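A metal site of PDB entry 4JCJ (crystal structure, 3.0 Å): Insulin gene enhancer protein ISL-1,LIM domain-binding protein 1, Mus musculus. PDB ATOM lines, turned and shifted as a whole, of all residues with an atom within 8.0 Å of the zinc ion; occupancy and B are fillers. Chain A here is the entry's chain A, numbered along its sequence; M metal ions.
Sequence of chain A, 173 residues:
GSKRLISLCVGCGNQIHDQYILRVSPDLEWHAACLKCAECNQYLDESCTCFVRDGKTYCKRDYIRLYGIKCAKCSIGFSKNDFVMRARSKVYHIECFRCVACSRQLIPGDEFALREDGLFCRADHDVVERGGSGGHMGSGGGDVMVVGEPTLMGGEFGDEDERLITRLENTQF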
ATOM      1  N   LEU A   8      -1.459 -29.954 -11.515  1.00  0.00           N
ATOM      2  CA  LEU A   8      -1.391 -30.439 -12.888  1.00  0.00           C
ATOM      3  C   LEU A   8      -1.340 -29.267 -13.848  1.00  0.00           C
ATOM      4  O   LEU A   8      -2.248 -28.436 -13.884  1.00  0.00           O
ATOM      5  CB  LEU A   8      -2.590 -31.354 -13.199  1.00  0.00           C
ATOM      6  N   CYS A   9      -0.275 -29.188 -14.632  1.00  0.00           N
ATOM      7  CA  CYS A   9      -0.103 -28.073 -15.562  1.00  0.00           C
ATOM      8  C   CYS A   9      -1.214 -28.027 -16.633  1.00  0.00           C
ATOM      9  O   CYS A   9      -1.382 -28.951 -17.424  1.00  0.00           O
ATOM     10  CB  CYS A   9       1.255 -28.168 -16.244  1.00  0.00           C
ATOM     11  SG  CYS A   9       1.338 -27.236 -17.725  1.00  0.00           S
ATOM     12  N   VAL A  10      -1.964 -26.934 -16.663  1.00  0.00           N
ATOM     13  CA  VAL A  10      -3.132 -26.840 -17.536  1.00  0.00           C
ATOM     14  C   VAL A  10      -2.810 -26.958 -19.049  1.00  0.00           C
ATOM     15  O   VAL A  10      -3.664 -27.310 -19.869  1.00  0.00           O
ATOM     16  CB  VAL A  10      -3.948 -25.534 -17.233  1.00  0.00           C
ATOM     17  CG1 VAL A  10      -4.873 -25.169 -18.381  1.00  0.00           C
ATOM     18  CG2 VAL A  10      -4.761 -25.720 -15.939  1.00  0.00           C
ATOM     19  N   GLY A  11      -1.570 -26.661 -19.415  1.00  0.00           N
ATOM     20  CA  GLY A  11      -1.167 -26.664 -20.804  1.00  0.00           C
ATOM     21  C   GLY A  11      -1.045 -28.075 -21.329  1.00  0.00           C
ATOM     22  O   GLY A  11      -1.534 -28.374 -22.429  1.00  0.00           O
ATOM     23  N   CYS A  12      -0.392 -28.917 -20.527  1.00  0.00           N
ATOM     24  CA  CYS A  12       0.012 -30.261 -20.940  1.00  0.00           C
ATOM     25  C   CYS A  12      -0.512 -31.381 -20.054  1.00  0.00           C
ATOM     26  O   CYS A  12      -0.298 -32.533 -20.362  1.00  0.00           O
ATOM     27  CB  CYS A  12       1.533 -30.348 -20.956  1.00  0.00           C
ATOM     28  SG  CYS A  12       2.304 -30.284 -19.321  1.00  0.00           S
ATOM     29  N   GLY A  13      -1.133 -31.042 -18.935  1.00  0.00           N
ATOM     30  CA  GLY A  13      -1.747 -32.022 -18.043  1.00  0.00           C
ATOM     31  C   GLY A  13      -0.842 -32.754 -17.049  1.00  0.00           C
ATOM     32  O   GLY A  13      -1.359 -33.434 -16.171  1.00  0.00           O
ATOM     33  N   ASN A  14       0.475 -32.627 -17.180  1.00  0.00           N
ATOM     34  CA  ASN A  14       1.408 -33.364 -16.317  1.00  0.00           C
ATOM     35  C   ASN A  14       1.727 -32.619 -15.032  1.00  0.00           C
ATOM     36  O   ASN A  14       1.478 -31.417 -14.955  1.00  0.00           O
ATOM     37  CB  ASN A  14       2.716 -33.613 -17.072  1.00  0.00           C
ATOM     38  CG  ASN A  14       2.486 -34.299 -18.411  1.00  0.00           C
ATOM     39  OD1 ASN A  14       2.155 -35.496 -18.466  1.00  0.00           O
ATOM     40  ND2 ASN A  14       2.689 -33.561 -19.496  1.00  0.00           N
ATOM     41  N   GLN A  15       2.262 -33.313 -14.023  1.00  0.00           N
ATOM     42  CA  GLN A  15       2.612 -32.668 -12.734  1.00  0.00           C
ATOM     43  C   GLN A  15       3.689 -31.605 -12.938  1.00  0.00           C
ATOM     44  O   GLN A  15       4.565 -31.770 -13.769  1.00  0.00           O
ATOM     45  CB  GLN A  15       3.131 -33.672 -11.692  1.00  0.00           C
ATOM     46  N   ILE A  16       3.594 -30.504 -12.180  1.00  0.00           N
ATOM     47  CA  ILE A  16       4.605 -29.455 -12.212  1.00  0.00           C
ATOM     48  C   ILE A  16       5.628 -29.682 -11.121  1.00  0.00           C
ATOM     49  O   ILE A  16       5.310 -29.537  -9.949  1.00  0.00           O
ATOM     50  CB  ILE A  16       3.987 -28.041 -12.007  1.00  0.00           C
ATOM     51  CG1 ILE A  16       2.884 -27.773 -13.028  1.00  0.00           C
ATOM     52  CG2 ILE A  16       5.075 -26.975 -12.131  1.00  0.00           C
ATOM     53  CD1 ILE A  16       2.371 -26.327 -13.057  1.00  0.00           C
ATOM     54  N   ASP A  18       8.695 -28.000 -11.087  1.00  0.00           N
ATOM     55  CA  ASP A  18       9.635 -26.872 -11.121  1.00  0.00           C
ATOM     56  C   ASP A  18       9.656 -26.176  -9.758  1.00  0.00           C
ATOM     57  O   ASP A  18       8.784 -26.421  -8.931  1.00  0.00           O
ATOM     58  CB  ASP A  18       9.246 -25.858 -12.196  1.00  0.00           C
ATOM     59  CG  ASP A  18       9.164 -26.476 -13.601  1.00  0.00           C
ATOM     60  OD1 ASP A  18       9.867 -27.472 -13.874  1.00  0.00           O
ATOM     61  OD2 ASP A  18       8.393 -25.937 -14.439  1.00  0.00           O
ATOM     62  N   GLU A  29      -2.885 -23.130 -12.957  1.00  0.00           N
ATOM     63  CA  GLU A  29      -1.457 -23.344 -12.645  1.00  0.00           C
ATOM     64  C   GLU A  29      -0.747 -23.848 -13.899  1.00  0.00           C
ATOM     65  O   GLU A  29      -1.294 -24.683 -14.605  1.00  0.00           O
ATOM     66  CB  GLU A  29      -1.296 -24.357 -11.505  1.00  0.00           C
ATOM     67  N   TRP A  30       0.454 -23.337 -14.143  1.00  0.00           N
ATOM     68  CA  TRP A  30       1.183 -23.650 -15.375  1.00  0.00           C
ATOM     69  C   TRP A  30       2.640 -23.968 -15.170  1.00  0.00           C
ATOM     70  O   TRP A  30       3.300 -23.330 -14.377  1.00  0.00           O
ATOM     71  CB  TRP A  30       1.175 -22.456 -16.304  1.00  0.00           C
ATOM     72  CG  TRP A  30      -0.137 -22.077 -16.755  1.00  0.00           C
ATOM     73  CD1 TRP A  30      -0.992 -21.249 -16.132  1.00  0.00           C
ATOM     74  CD2 TRP A  30      -0.757 -22.481 -17.958  1.00  0.00           C
ATOM     75  NE1 TRP A  30      -2.138 -21.109 -16.867  1.00  0.00           N
ATOM     76  CE2 TRP A  30      -2.023 -21.874 -17.999  1.00  0.00           C
ATOM     77  CE3 TRP A  30      -0.380 -23.321 -19.012  1.00  0.00           C
ATOM     78  CZ2 TRP A  30      -2.912 -22.065 -19.055  1.00  0.00           C
ATOM     79  CZ3 TRP A  30      -1.259 -23.511 -20.049  1.00  0.00           C
ATOM     80  CH2 TRP A  30      -2.515 -22.893 -20.070  1.00  0.00           C
ATOM     81  N   HIS A  31       3.144 -24.925 -15.921  1.00  0.00           N
ATOM     82  CA  HIS A  31       4.559 -24.983 -16.216  1.00  0.00           C
ATOM     83  C   HIS A  31       4.896 -23.654 -16.837  1.00  0.00           C
ATOM     84  O   HIS A  31       4.096 -23.101 -17.585  1.00  0.00           O
ATOM     85  CB  HIS A  31       4.859 -26.083 -17.238  1.00  0.00           C
ATOM     86  CG  HIS A  31       4.892 -27.461 -16.662  1.00  0.00           C
ATOM     87  ND1 HIS A  31       4.368 -28.552 -17.309  1.00  0.00           N
ATOM     88  CD2 HIS A  31       5.378 -27.919 -15.492  1.00  0.00           C
ATOM     89  CE1 HIS A  31       4.532 -29.622 -16.568  1.00  0.00           C
ATOM     90  NE2 HIS A  31       5.151 -29.271 -15.453  1.00  0.00           N
ATOM     91  N   ALA A  32       6.077 -23.141 -16.550  1.00  0.00           N
ATOM     92  CA  ALA A  32       6.446 -21.839 -17.100  1.00  0.00           C
ATOM     93  C   ALA A  32       6.587 -21.888 -18.603  1.00  0.00           C
ATOM     94  O   ALA A  32       6.305 -20.897 -19.278  1.00  0.00           O
ATOM     95  CB  ALA A  32       7.714 -21.321 -16.475  1.00  0.00           C
ATOM     96  N   ALA A  33       7.007 -23.046 -19.104  1.00  0.00           N
ATOM     97  CA  ALA A  33       7.191 -23.272 -20.540  1.00  0.00           C
ATOM     98  C   ALA A  33       5.898 -23.505 -21.307  1.00  0.00           C
ATOM     99  O   ALA A  33       5.884 -23.405 -22.532  1.00  0.00           O
ATOM    100  CB  ALA A  33       8.097 -24.464 -20.769  1.00  0.00           C
ATOM    101  N   CYS A  34       4.814 -23.828 -20.612  1.00  0.00           N
ATOM    102  CA  CYS A  34       3.573 -24.127 -21.297  1.00  0.00           C
ATOM    103  C   CYS A  34       2.632 -22.936 -21.338  1.00  0.00           C
ATOM    104  O   CYS A  34       1.542 -23.030 -21.904  1.00  0.00           O
ATOM    105  CB  CYS A  34       2.886 -25.329 -20.655  1.00  0.00           C
ATOM    106  SG  CYS A  34       3.787 -26.907 -20.798  1.00  0.00           S
ATOM    107  N   LEU A  35       3.034 -21.818 -20.740  1.00  0.00           N
ATOM    108  CA  LEU A  35       2.204 -20.625 -20.753  1.00  0.00           C
ATOM    109  C   LEU A  35       2.552 -19.730 -21.967  1.00  0.00           C
ATOM    110  O   LEU A  35       3.276 -18.748 -21.850  1.00  0.00           O
ATOM    111  CB  LEU A  35       2.343 -19.879 -19.424  1.00  0.00           C
ATOM    112  CG  LEU A  35       1.249 -18.827 -19.146  1.00  0.00           C
ATOM    113  CD1 LEU A  35      -0.061 -19.501 -18.913  1.00  0.00           C
ATOM    114  CD2 LEU A  35       1.586 -18.015 -17.934  1.00  0.00           C
HETATM  115 ZN    ZN M   1       3.083 -28.130 -18.953  1.00  0.00          ZN
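O of Cys 12 lies within hydrogen-bond range of ND2 of Asn 14, at 3.3 Å.
The backbone carbonyl oxygen of Asn 14 lies within hydrogen-bond range of the backbone NH of Cys 9 (2.9 Å).
A ring nitrogen (NE2) of His 31 lies within hydrogen-bond range of the backbone carbonyl oxygen of Gln 15.
The backbone NH of Gly 11 sits close to the side-chain sulfur of Cys 9.
The zinc ion is bound by ND1 of His 31 (2.1 Å), SG of Cys 9 (2.3 Å), SG of Cys 12 (2.3 Å) and SG of Cys 34 (2.3 Å).
The zinc ion has four donor atoms within binding distance.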
